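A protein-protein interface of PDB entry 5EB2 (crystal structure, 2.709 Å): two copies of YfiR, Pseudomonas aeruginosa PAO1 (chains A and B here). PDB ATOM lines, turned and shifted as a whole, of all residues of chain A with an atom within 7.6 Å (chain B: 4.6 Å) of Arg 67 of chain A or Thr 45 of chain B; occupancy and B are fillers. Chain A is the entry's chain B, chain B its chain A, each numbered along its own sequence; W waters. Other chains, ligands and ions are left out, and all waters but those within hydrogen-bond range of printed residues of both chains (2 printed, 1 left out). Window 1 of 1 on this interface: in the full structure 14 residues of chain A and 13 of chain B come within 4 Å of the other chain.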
ATOM      1  N   LEU A  39       6.916 -13.430  -2.887  1.00  0.00           N
ATOM      2  CA  LEU A  39       5.729 -13.052  -3.656  1.00  0.00           C
ATOM      3  C   LEU A  39       5.772 -11.569  -3.995  1.00  0.00           C
ATOM      4  O   LEU A  39       5.986 -10.716  -3.116  1.00  0.00           O
ATOM      5  CB  LEU A  39       4.441 -13.386  -2.900  1.00  0.00           C
ATOM      6  CG  LEU A  39       3.112 -13.255  -3.676  1.00  0.00           C
ATOM      7  CD1 LEU A  39       2.035 -14.097  -3.032  1.00  0.00           C
ATOM      8  CD2 LEU A  39       2.617 -11.845  -3.775  1.00  0.00           C
ATOM      9  N   CYS A  40       5.545 -11.262  -5.268  1.00  0.00           N
ATOM     10  CA  CYS A  40       5.468  -9.870  -5.716  1.00  0.00           C
ATOM     11  C   CYS A  40       4.057  -9.464  -6.152  1.00  0.00           C
ATOM     12  O   CYS A  40       3.434 -10.107  -7.001  1.00  0.00           O
ATOM     13  CB  CYS A  40       6.437  -9.625  -6.868  1.00  0.00           C
ATOM     14  SG  CYS A  40       8.168  -9.846  -6.427  1.00  0.00           S
ATOM     15  N   VAL A  41       3.566  -8.379  -5.571  1.00  0.00           N
ATOM     16  CA  VAL A  41       2.307  -7.801  -6.004  1.00  0.00           C
ATOM     17  C   VAL A  41       2.590  -6.654  -6.967  1.00  0.00           C
ATOM     18  O   VAL A  41       3.265  -5.694  -6.616  1.00  0.00           O
ATOM     19  CB  VAL A  41       1.481  -7.310  -4.820  1.00  0.00           C
ATOM     20  CG1 VAL A  41       0.174  -6.737  -5.314  1.00  0.00           C
ATOM     21  CG2 VAL A  41       1.229  -8.467  -3.843  1.00  0.00           C
ATOM     22  N   VAL A  42       2.080  -6.778  -8.185  1.00  0.00           N
ATOM     23  CA  VAL A  42       2.436  -5.895  -9.286  1.00  0.00           C
ATOM     24  C   VAL A  42       1.188  -5.323  -9.936  1.00  0.00           C
ATOM     25  O   VAL A  42       0.340  -6.080 -10.435  1.00  0.00           O
ATOM     26  CB  VAL A  42       3.264  -6.638 -10.366  1.00  0.00           C
ATOM     27  CG1 VAL A  42       3.514  -5.740 -11.556  1.00  0.00           C
ATOM     28  CG2 VAL A  42       4.579  -7.146  -9.794  1.00  0.00           C
ATOM     29  N   GLY A  43       1.081  -3.994  -9.943  1.00  0.00           N
ATOM     30  CA  GLY A  43      -0.084  -3.334 -10.498  1.00  0.00           C
ATOM     31  C   GLY A  43      -1.143  -3.010  -9.454  1.00  0.00           C
ATOM     32  O   GLY A  43      -1.065  -3.448  -8.315  1.00  0.00           O
ATOM     33  N   PRO A  44      -2.136  -2.207  -9.835  1.00  0.00           N
ATOM     34  CA  PRO A  44      -3.265  -1.924  -8.943  1.00  0.00           C
ATOM     35  C   PRO A  44      -4.033  -3.183  -8.588  1.00  0.00           C
ATOM     36  O   PRO A  44      -4.425  -3.944  -9.481  1.00  0.00           O
ATOM     37  CB  PRO A  44      -4.143  -0.985  -9.773  1.00  0.00           C
ATOM     38  CG  PRO A  44      -3.192  -0.346 -10.744  1.00  0.00           C
ATOM     39  CD  PRO A  44      -2.150  -1.366 -11.046  1.00  0.00           C
ATOM     40  N   THR A  45      -4.259  -3.388  -7.298  1.00  0.00           N
ATOM     41  CA  THR A  45      -5.012  -4.540  -6.807  1.00  0.00           C
ATOM     42  C   THR A  45      -6.015  -4.107  -5.754  1.00  0.00           C
ATOM     43  O   THR A  45      -5.828  -3.102  -5.071  1.00  0.00           O
ATOM     44  CB  THR A  45      -4.094  -5.594  -6.177  1.00  0.00           C
ATOM     45  OG1 THR A  45      -3.359  -4.979  -5.105  1.00  0.00           O
ATOM     46  CG2 THR A  45      -3.120  -6.170  -7.210  1.00  0.00           C
ATOM     47  N   GLU A  46      -7.061  -4.899  -5.597  1.00  0.00           N
ATOM     48  CA  GLU A  46      -8.142  -4.594  -4.674  1.00  0.00           C
ATOM     49  C   GLU A  46      -8.123  -5.575  -3.489  1.00  0.00           C
ATOM     50  O   GLU A  46      -8.567  -5.255  -2.396  1.00  0.00           O
ATOM     51  CB  GLU A  46      -9.462  -4.654  -5.452  1.00  0.00           C
ATOM     52  CG  GLU A  46     -10.687  -4.052  -4.807  1.00  0.00           C
ATOM     53  CD  GLU A  46     -11.870  -3.935  -5.777  1.00  0.00           C
ATOM     54  OE1 GLU A  46     -12.870  -3.276  -5.404  1.00  0.00           O
ATOM     55  OE2 GLU A  46     -11.805  -4.498  -6.905  1.00  0.00           O
ATOM     56  N   TYR A  47      -7.570  -6.770  -3.707  1.00  0.00           N
ATOM     57  CA  TYR A  47      -7.712  -7.874  -2.752  1.00  0.00           C
ATOM     58  C   TYR A  47      -6.373  -8.455  -2.256  1.00  0.00           C
ATOM     59  O   TYR A  47      -6.318  -9.581  -1.749  1.00  0.00           O
ATOM     60  CB  TYR A  47      -8.543  -9.002  -3.373  1.00  0.00           C
ATOM     61  CG  TYR A  47      -9.915  -8.609  -3.856  1.00  0.00           C
ATOM     62  CD1 TYR A  47     -10.958  -8.373  -2.954  1.00  0.00           C
ATOM     63  CD2 TYR A  47     -10.189  -8.511  -5.218  1.00  0.00           C
ATOM     64  CE1 TYR A  47     -12.228  -8.028  -3.395  1.00  0.00           C
ATOM     65  CE2 TYR A  47     -11.465  -8.175  -5.673  1.00  0.00           C
ATOM     66  CZ  TYR A  47     -12.478  -7.928  -4.756  1.00  0.00           C
ATOM     67  OH  TYR A  47     -13.741  -7.579  -5.203  1.00  0.00           O
ATOM     68  N   ALA A  48      -5.304  -7.684  -2.384  1.00  0.00           N
ATOM     69  CA  ALA A  48      -3.985  -8.161  -2.005  1.00  0.00           C
ATOM     70  C   ALA A  48      -3.523  -7.739  -0.591  1.00  0.00           C
ATOM     71  O   ALA A  48      -2.384  -8.028  -0.207  1.00  0.00           O
ATOM     72  CB  ALA A  48      -2.977  -7.705  -3.040  1.00  0.00           C
ATOM     73  N   ASP A  49      -4.374  -7.096   0.211  1.00  0.00           N
ATOM     74  CA  ASP A  49      -3.876  -6.621   1.520  1.00  0.00           C
ATOM     75  C   ASP A  49      -3.539  -7.755   2.485  1.00  0.00           C
ATOM     76  O   ASP A  49      -2.728  -7.566   3.386  1.00  0.00           O
ATOM     77  CB  ASP A  49      -4.861  -5.672   2.193  1.00  0.00           C
ATOM     78  CG  ASP A  49      -4.969  -4.344   1.480  1.00  0.00           C
ATOM     79  OD1 ASP A  49      -4.137  -4.083   0.580  1.00  0.00           O
ATOM     80  OD2 ASP A  49      -5.883  -3.557   1.821  1.00  0.00           O
ATOM     81  N   LEU A  52      -0.073  -9.161   1.513  1.00  0.00           N
ATOM     82  CA  LEU A  52       1.011  -8.242   1.852  1.00  0.00           C
ATOM     83  C   LEU A  52       1.399  -8.305   3.320  1.00  0.00           C
ATOM     84  O   LEU A  52       2.513  -7.935   3.674  1.00  0.00           O
ATOM     85  CB  LEU A  52       0.649  -6.821   1.450  1.00  0.00           C
ATOM     86  CG  LEU A  52       0.666  -6.705  -0.076  1.00  0.00           C
ATOM     87  CD1 LEU A  52       0.032  -5.410  -0.520  1.00  0.00           C
ATOM     88  CD2 LEU A  52       2.089  -6.858  -0.640  1.00  0.00           C
ATOM     89  N   HIS A  64       7.122 -14.162   1.809  1.00  0.00           N
ATOM     90  CA  HIS A  64       7.365 -12.752   1.950  1.00  0.00           C
ATOM     91  C   HIS A  64       6.772 -11.999   0.775  1.00  0.00           C
ATOM     92  O   HIS A  64       7.133 -12.251  -0.375  1.00  0.00           O
ATOM     93  CB  HIS A  64       8.858 -12.462   2.038  1.00  0.00           C
ATOM     94  CG  HIS A  64       9.153 -11.002   2.122  1.00  0.00           C
ATOM     95  ND1 HIS A  64       8.906 -10.267   3.260  1.00  0.00           N
ATOM     96  CD2 HIS A  64       9.594 -10.126   1.189  1.00  0.00           C
ATOM     97  CE1 HIS A  64       9.213  -9.002   3.035  1.00  0.00           C
ATOM     98  NE2 HIS A  64       9.637  -8.890   1.786  1.00  0.00           N
ATOM     99  N   ALA A  65       5.885 -11.056   1.058  1.00  0.00           N
ATOM    100  CA  ALA A  65       5.211 -10.341  -0.017  1.00  0.00           C
ATOM    101  C   ALA A  65       5.618  -8.871  -0.060  1.00  0.00           C
ATOM    102  O   ALA A  65       5.850  -8.266   0.974  1.00  0.00           O
ATOM    103  CB  ALA A  65       3.717 -10.476   0.138  1.00  0.00           C
ATOM    104  N   GLU A  66       5.711  -8.313  -1.265  1.00  0.00           N
ATOM    105  CA  GLU A  66       6.123  -6.927  -1.477  1.00  0.00           C
ATOM    106  C   GLU A  66       5.530  -6.408  -2.773  1.00  0.00           C
ATOM    107  O   GLU A  66       5.434  -7.164  -3.742  1.00  0.00           O
ATOM    108  CB  GLU A  66       7.642  -6.816  -1.555  1.00  0.00           C
ATOM    109  CG  GLU A  66       8.289  -6.153  -0.366  1.00  0.00           C
ATOM    110  CD  GLU A  66       9.801  -6.233  -0.430  1.00  0.00           C
ATOM    111  OE1 GLU A  66      10.321  -6.815  -1.410  1.00  0.00           O
ATOM    112  OE2 GLU A  66      10.462  -5.718   0.500  1.00  0.00           O
ATOM    113  N   ARG A  67       5.153  -5.132  -2.821  1.00  0.00           N
ATOM    114  CA  ARG A  67       4.801  -4.546  -4.102  1.00  0.00           C
ATOM    115  C   ARG A  67       6.041  -4.268  -4.917  1.00  0.00           C
ATOM    116  O   ARG A  67       7.094  -3.903  -4.376  1.00  0.00           O
ATOM    117  CB  ARG A  67       4.018  -3.255  -3.932  1.00  0.00           C
ATOM    118  CG  ARG A  67       2.608  -3.472  -3.485  1.00  0.00           C
ATOM    119  CD  ARG A  67       1.819  -2.182  -3.470  1.00  0.00           C
ATOM    120  NE  ARG A  67       0.442  -2.475  -3.111  1.00  0.00           N
ATOM    121  CZ  ARG A  67      -0.439  -2.962  -3.976  1.00  0.00           C
ATOM    122  NH1 ARG A  67      -0.076  -3.197  -5.247  1.00  0.00           N
ATOM    123  NH2 ARG A  67      -1.672  -3.213  -3.575  1.00  0.00           N
ATOM    124  N   ARG A  68       5.917  -4.444  -6.227  1.00  0.00           N
ATOM    125  CA  ARG A  68       6.963  -4.019  -7.147  1.00  0.00           C
ATOM    126  C   ARG A  68       6.307  -3.344  -8.341  1.00  0.00           C
ATOM    127  O   ARG A  68       5.153  -3.610  -8.648  1.00  0.00           O
ATOM    128  CB  ARG A  68       7.848  -5.195  -7.591  1.00  0.00           C
ATOM    129  CG  ARG A  68       8.431  -6.011  -6.457  1.00  0.00           C
ATOM    130  CD  ARG A  68       9.945  -5.913  -6.380  1.00  0.00           C
ATOM    131  NE  ARG A  68      10.436  -6.656  -5.221  1.00  0.00           N
ATOM    132  CZ  ARG A  68      11.604  -6.447  -4.623  1.00  0.00           C
ATOM    133  NH1 ARG A  68      12.424  -5.510  -5.071  1.00  0.00           N
ATOM    134  NH2 ARG A  68      11.953  -7.175  -3.568  1.00  0.00           N
ATOM    135  N   ALA A  69       7.046  -2.452  -8.990  1.00  0.00           N
ATOM    136  CA  ALA A  69       6.528  -1.651 -10.097  1.00  0.00           C
ATOM    137  C   ALA A  69       6.380  -2.463 -11.384  1.00  0.00           C
ATOM    138  O   ALA A  69       7.153  -3.379 -11.635  1.00  0.00           O
ATOM    139  CB  ALA A  69       7.427  -0.463 -10.333  1.00  0.00           C
ATOM    140  N   ASN A  72       9.504  -2.625 -13.447  1.00  0.00           N
ATOM    141  CA  ASN A  72      10.693  -3.207 -12.828  1.00  0.00           C
ATOM    142  C   ASN A  72      11.226  -4.335 -13.716  1.00  0.00           C
ATOM    143  O   ASN A  72      10.575  -5.362 -13.885  1.00  0.00           O
ATOM    144  CB  ASN A  72      10.373  -3.714 -11.412  1.00  0.00           C
ATOM    145  CG  ASN A  72      11.621  -4.049 -10.602  1.00  0.00           C
ATOM    146  OD1 ASN A  72      12.619  -4.533 -11.142  1.00  0.00           O
ATOM    147  ND2 ASN A  72      11.567  -3.790  -9.292  1.00  0.00           N
ATOM    148  N   LEU A  75      11.766  -8.385 -12.432  1.00  0.00           N
ATOM    149  CA  LEU A  75      10.660  -9.131 -11.828  1.00  0.00           C
ATOM    150  C   LEU A  75      10.890 -10.629 -11.905  1.00  0.00           C
ATOM    151  O   LEU A  75      10.547 -11.350 -10.979  1.00  0.00           O
ATOM    152  CB  LEU A  75       9.324  -8.793 -12.494  1.00  0.00           C
ATOM    153  CG  LEU A  75       8.667  -7.423 -12.315  1.00  0.00           C
ATOM    154  CD1 LEU A  75       7.318  -7.405 -13.021  1.00  0.00           C
ATOM    155  CD2 LEU A  75       8.513  -7.060 -10.855  1.00  0.00           C
ATOM    156  N   CYS A  79      11.127 -12.413  -8.139  1.00  0.00           N
ATOM    157  CA  CYS A  79       9.855 -13.012  -7.751  1.00  0.00           C
ATOM    158  C   CYS A  79       9.854 -14.516  -7.959  1.00  0.00           C
ATOM    159  O   CYS A  79      10.395 -15.013  -8.941  1.00  0.00           O
ATOM    160  CB  CYS A  79       8.707 -12.379  -8.547  1.00  0.00           C
ATOM    161  SG  CYS A  79       8.548 -10.565  -8.299  1.00  0.00           S
ATOM    162  N   TYR A  83       1.718 -11.764  -8.370  1.00  0.00           N
ATOM    163  CA  TYR A  83       0.294 -11.590  -8.282  1.00  0.00           C
ATOM    164  C   TYR A  83       0.003 -10.333  -9.082  1.00  0.00           C
ATOM    165  O   TYR A  83       0.408  -9.243  -8.691  1.00  0.00           O
ATOM    166  CB  TYR A  83      -0.140 -11.478  -6.822  1.00  0.00           C
ATOM    167  CG  TYR A  83      -1.617 -11.277  -6.601  1.00  0.00           C
ATOM    168  CD1 TYR A  83      -2.490 -12.363  -6.523  1.00  0.00           C
ATOM    169  CD2 TYR A  83      -2.147  -9.992  -6.458  1.00  0.00           C
ATOM    170  CE1 TYR A  83      -3.841 -12.174  -6.311  1.00  0.00           C
ATOM    171  CE2 TYR A  83      -3.492  -9.791  -6.240  1.00  0.00           C
ATOM    172  CZ  TYR A  83      -4.334 -10.883  -6.169  1.00  0.00           C
ATOM    173  OH  TYR A  83      -5.672 -10.676  -5.955  1.00  0.00           O
ATOM    174  N   GLY A  85      -2.056  -7.356 -10.872  1.00  0.00           N
ATOM    175  CA  GLY A  85      -3.254  -6.534 -10.821  1.00  0.00           C
ATOM    176  C   GLY A  85      -3.561  -5.936 -12.183  1.00  0.00           C
ATOM    177  O   GLY A  85      -3.135  -6.446 -13.209  1.00  0.00           O
ATOM    178  N   VAL A  86      -4.296  -4.835 -12.198  1.00  0.00           N
ATOM    179  CA  VAL A  86      -4.713  -4.209 -13.449  1.00  0.00           C
ATOM    180  C   VAL A  86      -3.542  -3.645 -14.268  1.00  0.00           C
ATOM    181  O   VAL A  86      -2.797  -2.787 -13.803  1.00  0.00           O
ATOM    182  CB  VAL A  86      -5.729  -3.080 -13.169  1.00  0.00           C
ATOM    183  CG1 VAL A  86      -5.894  -2.166 -14.387  1.00  0.00           C
ATOM    184  CG2 VAL A  86      -7.062  -3.672 -12.740  1.00  0.00           C
ATOM    185  N   GLU A 109      -5.357 -11.075 -10.522  1.00  0.00           N
ATOM    186  CA  GLU A 109      -6.517 -10.847  -9.675  1.00  0.00           C
ATOM    187  C   GLU A 109      -7.842 -10.870 -10.460  1.00  0.00           C
ATOM    188  O   GLU A 109      -8.872 -11.246  -9.915  1.00  0.00           O
ATOM    189  CB  GLU A 109      -6.345  -9.513  -8.936  1.00  0.00           C
ATOM    190  CG  GLU A 109      -7.532  -9.088  -8.105  1.00  0.00           C
ATOM    191  CD  GLU A 109      -7.261  -7.840  -7.305  1.00  0.00           C
ATOM    192  OE1 GLU A 109      -6.839  -7.968  -6.142  1.00  0.00           O
ATOM    193  OE2 GLU A 109      -7.464  -6.728  -7.830  1.00  0.00           O
ATOM    194  N   ILE B  10       8.107   1.827  -5.180  1.00  0.00           N
ATOM    195  CA  ILE B  10       6.691   1.723  -4.809  1.00  0.00           C
ATOM    196  C   ILE B  10       6.471   2.102  -3.350  1.00  0.00           C
ATOM    197  O   ILE B  10       5.473   2.728  -3.011  1.00  0.00           O
ATOM    198  CB  ILE B  10       6.106   0.310  -5.059  1.00  0.00           C
ATOM    199  CG1 ILE B  10       6.159  -0.025  -6.536  1.00  0.00           C
ATOM    200  CG2 ILE B  10       4.614   0.264  -4.705  1.00  0.00           C
ATOM    201  CD1 ILE B  10       5.274   0.897  -7.359  1.00  0.00           C
ATOM    202  N   VAL B  41     -10.869   3.522   0.608  1.00  0.00           N
ATOM    203  CA  VAL B  41     -10.138   3.214  -0.618  1.00  0.00           C
ATOM    204  C   VAL B  41     -11.029   2.343  -1.503  1.00  0.00           C
ATOM    205  O   VAL B  41     -11.491   1.280  -1.089  1.00  0.00           O
ATOM    206  CB  VAL B  41      -8.798   2.504  -0.307  1.00  0.00           C
ATOM    207  CG1 VAL B  41      -8.073   2.080  -1.587  1.00  0.00           C
ATOM    208  CG2 VAL B  41      -7.927   3.408   0.525  1.00  0.00           C
ATOM    209  N   GLY B  43     -11.719   0.486  -5.275  1.00  0.00           N
ATOM    210  CA  GLY B  43     -11.128   0.030  -6.523  1.00  0.00           C
ATOM    211  C   GLY B  43      -9.665  -0.343  -6.352  1.00  0.00           C
ATOM    212  O   GLY B  43      -9.060  -0.020  -5.336  1.00  0.00           O
ATOM    213  N   PRO B  44      -9.088  -1.038  -7.343  1.00  0.00           N
ATOM    214  CA  PRO B  44      -7.686  -1.474  -7.272  1.00  0.00           C
ATOM    215  C   PRO B  44      -6.749  -0.292  -7.151  1.00  0.00           C
ATOM    216  O   PRO B  44      -6.919   0.690  -7.875  1.00  0.00           O
ATOM    217  CB  PRO B  44      -7.457  -2.193  -8.598  1.00  0.00           C
ATOM    218  CG  PRO B  44      -8.831  -2.500  -9.121  1.00  0.00           C
ATOM    219  CD  PRO B  44      -9.725  -1.417  -8.612  1.00  0.00           C
ATOM    220  N   THR B  45      -5.780  -0.376  -6.245  1.00  0.00           N
ATOM    221  CA  THR B  45      -4.822   0.703  -6.073  1.00  0.00           C
ATOM    222  C   THR B  45      -3.416   0.157  -5.913  1.00  0.00           C
ATOM    223  O   THR B  45      -3.206  -0.915  -5.357  1.00  0.00           O
ATOM    224  CB  THR B  45      -5.149   1.578  -4.841  1.00  0.00           C
ATOM    225  OG1 THR B  45      -5.159   0.752  -3.674  1.00  0.00           O
ATOM    226  CG2 THR B  45      -6.501   2.241  -4.979  1.00  0.00           C
ATOM    227  N   GLU B  46      -2.451   0.929  -6.382  1.00  0.00           N
ATOM    228  CA  GLU B  46      -1.049   0.572  -6.288  1.00  0.00           C
ATOM    229  C   GLU B  46      -0.391   1.237  -5.070  1.00  0.00           C
ATOM    230  O   GLU B  46       0.558   0.679  -4.505  1.00  0.00           O
ATOM    231  CB  GLU B  46      -0.342   0.984  -7.585  1.00  0.00           C
ATOM    232  CG  GLU B  46       0.889   0.228  -7.937  1.00  0.00           C
ATOM    233  CD  GLU B  46       1.255   0.384  -9.408  1.00  0.00           C
ATOM    234  OE1 GLU B  46       2.329  -0.142  -9.820  1.00  0.00           O
ATOM    235  OE2 GLU B  46       0.463   1.031 -10.148  1.00  0.00           O
ATOM    236  N   TYR B  47      -0.911   2.405  -4.661  1.00  0.00           N
ATOM    237  CA  TYR B  47      -0.198   3.339  -3.770  1.00  0.00           C
ATOM    238  C   TYR B  47      -0.917   3.684  -2.472  1.00  0.00           C
ATOM    239  O   TYR B  47      -0.605   4.695  -1.829  1.00  0.00           O
ATOM    240  CB  TYR B  47       0.103   4.659  -4.502  1.00  0.00           C
ATOM    241  CG  TYR B  47       0.961   4.464  -5.717  1.00  0.00           C
ATOM    242  CD1 TYR B  47       2.250   3.956  -5.599  1.00  0.00           C
ATOM    243  CD2 TYR B  47       0.495   4.790  -6.983  1.00  0.00           C
ATOM    244  CE1 TYR B  47       3.048   3.763  -6.713  1.00  0.00           C
ATOM    245  CE2 TYR B  47       1.287   4.591  -8.105  1.00  0.00           C
ATOM    246  CZ  TYR B  47       2.561   4.074  -7.965  1.00  0.00           C
ATOM    247  OH  TYR B  47       3.352   3.876  -9.086  1.00  0.00           O
ATOM    248  N   ALA B  48      -1.862   2.849  -2.078  1.00  0.00           N
ATOM    249  CA  ALA B  48      -2.676   3.136  -0.916  1.00  0.00           C
ATOM    250  C   ALA B  48      -2.247   2.359   0.348  1.00  0.00           C
ATOM    251  O   ALA B  48      -2.866   2.511   1.408  1.00  0.00           O
ATOM    252  CB  ALA B  48      -4.123   2.845  -1.241  1.00  0.00           C
ATOM    253  N   ASP B  49      -1.212   1.529   0.253  1.00  0.00           N
ATOM    254  CA  ASP B  49      -0.852   0.686   1.399  1.00  0.00           C
ATOM    255  C   ASP B  49      -0.416   1.531   2.610  1.00  0.00           C
ATOM    256  O   ASP B  49      -0.601   1.116   3.756  1.00  0.00           O
ATOM    257  CB  ASP B  49       0.238  -0.331   1.022  1.00  0.00           C
ATOM    258  CG  ASP B  49      -0.262  -1.399   0.025  1.00  0.00           C
ATOM    259  OD1 ASP B  49      -1.474  -1.402  -0.293  1.00  0.00           O
ATOM    260  OD2 ASP B  49       0.555  -2.234  -0.450  1.00  0.00           O
ATOM    261  N   ARG B  67     -10.774  -0.378   2.778  1.00  0.00           N
ATOM    262  CA  ARG B  67     -11.218  -0.556   1.410  1.00  0.00           C
ATOM    263  C   ARG B  67     -12.704  -0.780   1.425  1.00  0.00           C
ATOM    264  O   ARG B  67     -13.216  -1.417   2.340  1.00  0.00           O
ATOM    265  CB  ARG B  67     -10.512  -1.738   0.745  1.00  0.00           C
ATOM    266  CG  ARG B  67      -9.009  -1.772   0.943  1.00  0.00           C
ATOM    267  CD  ARG B  67      -8.322  -2.768  -0.004  1.00  0.00           C
ATOM    268  NE  ARG B  67      -7.944  -2.129  -1.255  1.00  0.00           N
ATOM    269  CZ  ARG B  67      -6.697  -1.798  -1.562  1.00  0.00           C
ATOM    270  NH1 ARG B  67      -5.715  -2.076  -0.713  1.00  0.00           N
ATOM    271  NH2 ARG B  67      -6.432  -1.201  -2.721  1.00  0.00           N
ATOM    272  N   TYR B  83     -10.596   7.650  -1.691  1.00  0.00           N
ATOM    273  CA  TYR B  83      -9.381   7.531  -2.499  1.00  0.00           C
ATOM    274  C   TYR B  83      -9.707   6.493  -3.579  1.00  0.00           C
ATOM    275  O   TYR B  83      -9.970   5.319  -3.282  1.00  0.00           O
ATOM    276  CB  TYR B  83      -8.173   7.150  -1.641  1.00  0.00           C
ATOM    277  CG  TYR B  83      -6.882   6.979  -2.398  1.00  0.00           C
ATOM    278  CD1 TYR B  83      -6.033   8.056  -2.622  1.00  0.00           C
ATOM    279  CD2 TYR B  83      -6.493   5.726  -2.879  1.00  0.00           C
ATOM    280  CE1 TYR B  83      -4.842   7.907  -3.322  1.00  0.00           C
ATOM    281  CE2 TYR B  83      -5.306   5.559  -3.567  1.00  0.00           C
ATOM    282  CZ  TYR B  83      -4.482   6.656  -3.785  1.00  0.00           C
ATOM    283  OH  TYR B  83      -3.305   6.485  -4.482  1.00  0.00           O
ATOM    284  N   GLY B  85      -9.457   4.255  -7.077  1.00  0.00           N
ATOM    285  CA  GLY B  85      -8.507   3.540  -7.894  1.00  0.00           C
ATOM    286  C   GLY B  85      -9.007   3.388  -9.304  1.00  0.00           C
ATOM    287  O   GLY B  85      -9.642   4.281  -9.867  1.00  0.00           O
ATOM    288  N   GLU B 109      -6.087   8.121  -7.532  1.00  0.00           N
ATOM    289  CA  GLU B 109      -4.702   7.704  -7.635  1.00  0.00           C
ATOM    290  C   GLU B 109      -4.136   8.103  -8.999  1.00  0.00           C
ATOM    291  O   GLU B 109      -2.970   8.474  -9.109  1.00  0.00           O
ATOM    292  CB  GLU B 109      -4.582   6.195  -7.418  1.00  0.00           C
ATOM    293  CG  GLU B 109      -3.158   5.650  -7.526  1.00  0.00           C
ATOM    294  CD  GLU B 109      -3.039   4.236  -6.987  1.00  0.00           C
ATOM    295  OE1 GLU B 109      -3.071   4.079  -5.745  1.00  0.00           O
ATOM    296  OE2 GLU B 109      -2.925   3.290  -7.805  1.00  0.00           O
HETATM  297  O   HOH W   1     -12.270  -1.653  -3.503  1.00  0.00           O
HETATM  298  O   HOH W   2      -2.783  -0.294  -2.571  1.00  0.00           O
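Of the 25 printed residues of chain A, 8 touch a printed residue of chain B. Printed residues of chain A that touch a printed residue of chain B: Pro 44, Thr 45, Glu 46, Asp 49, Leu 52, Arg 67, Arg 68 and Ala 69. Hydrophobic or aromatic side chains of chain A that line the printed part of chain B: Pro 44, Leu 52 and Ala 69. Along chain B the printed residues that touch a printed residue of chain A span positions 10 to 67. Among the printed residues, Asp or Glu carboxylates within 4 Å of a Lys or Arg side-chain nitrogen of the other chain: Asp 49 of chain A with Arg 67 of chain B (2.9 Å) and Arg 67 of chain A with Asp 49 of chain B (2.7 Å).
Pro 44 of chain B touches Pro 44 of chain A (CB to C, 3.6 Å). Thr 45 of chain B touches Pro 44 of chain A (C to CA, 3.7 Å). Glu 46 of chain A touches Gly 43 of chain B. N of Glu 46 of chain A touches CA of Pro 44 of chain B (3.9 Å). Asp 49 of chain A touches Asp 49 of chain B. Leu 52 of chain A touches Asp 49 of chain B. Ala 69 of chain A touches Ile 10 of chain B (N to CG1, 3.6 Å).
The backbone carbonyl oxygen of Glu 46 of chain A sits at hydrogen-bond distance from the guanidinium group of Arg 67 of chain B, 3.4 Å away. The backbone carbonyl oxygen (O) of Thr 45 of chain B sits at hydrogen-bond distance from the guanidinium group (NH2) of Arg 67 of chain A (3.3 Å). The backbone carbonyl oxygen (O) of Thr 45 of chain A is in hydrogen-bond range of the backbone NH (N) of Thr 45 of chain B (3.0 Å). The guanidinium group of Arg 67 of chain A is in salt-bridge range of the side-chain carboxylate of Asp 49 of chain B. O of Glu 46 of chain B sits close to NE of Arg 67 of chain A (3.5 Å). OD1 of Asp 49 of chain A lies within salt-bridge range of NH1 of Arg 67 of chain B, 2.9 Å away. The guanidinium group (NH2) of Arg 67 of chain B lies within hydrogen-bond range of the backbone carbonyl oxygen (O) of Thr 45 of chain A (3.1 Å).
Printed residues of chain B within 4 Å of Asp 49 of chain A: Asp 49 (3.9 Å) and Arg 67 (2.9 Å). Of chain B, only Ile 10, Thr 45, Glu 46 and Asp 49 come within 4 Å of Arg 67 of chain A. Printed residues of chain B within 4 Å of Ala 69 of chain A: Ile 10. Of the printed residues of chain A, Ile 10 of chain B touches Arg 67 (3.7 Å), Arg 68 (3.8 Å) and Ala 69 (3.6 Å). Gly 85 of chain B touches none of the printed residues of chain A. The nearest printed residue of chain B that does not touch Arg 67 of chain A is Arg 67 of chain B (5.1 Å). The nearest residue of chain A that does not touch Thr 45 of chain B is Gly 43 of chain A (4.4 Å). The nearest printed residue of chain B that does not touch Glu 46 of chain A is Thr 45 of chain B (4.7 Å).
Water W1 lies within hydrogen-bond range of OE1 of Glu 46 of chain A (2.6 Å) and N of Gly 43 of chain B (2.8 Å). Water W2 lies within hydrogen-bond range of the side-chain hydroxyl (OG1) of Thr 45 of chain B, the side-chain carboxylate (OD1) of Asp 49 of chain B, the guanidinium group (NH2) of Arg 67 of chain A and the backbone NH (N) of Ala 48 of chain B.
The backbone carbonyl oxygen (O) of Pro 44 of chain A is in hydrogen-bond range of the backbone NH (N) of Val 86 of chain A, 2.9 Å away. The guanidinium group (NH1) of Arg 67 of chain A sits at hydrogen-bond distance from the backbone carbonyl oxygen (O) of Gly 43 of chain A (3.2 Å). The backbone NH (N) of Glu 46 of chain B is in hydrogen-bond range of the side-chain carboxylate (OE2) of Glu 109 of chain B.
Pro 44 of chain B touches its own counterpart, Pro 44 of chain A. Pro 44 of chain A touches Thr 45 of chain B, and with the chains exchanged Thr 45 of chain A touches Pro 44 of chain B. Thr 45 of chain A touches Arg 67 of chain B, and with the chains exchanged Arg 67 of chain A touches Thr 45 of chain B. Positions printed for both chains: 41, 43, 44, 45, 46, 47, 48, 49, 67, 83, 85 and 109.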
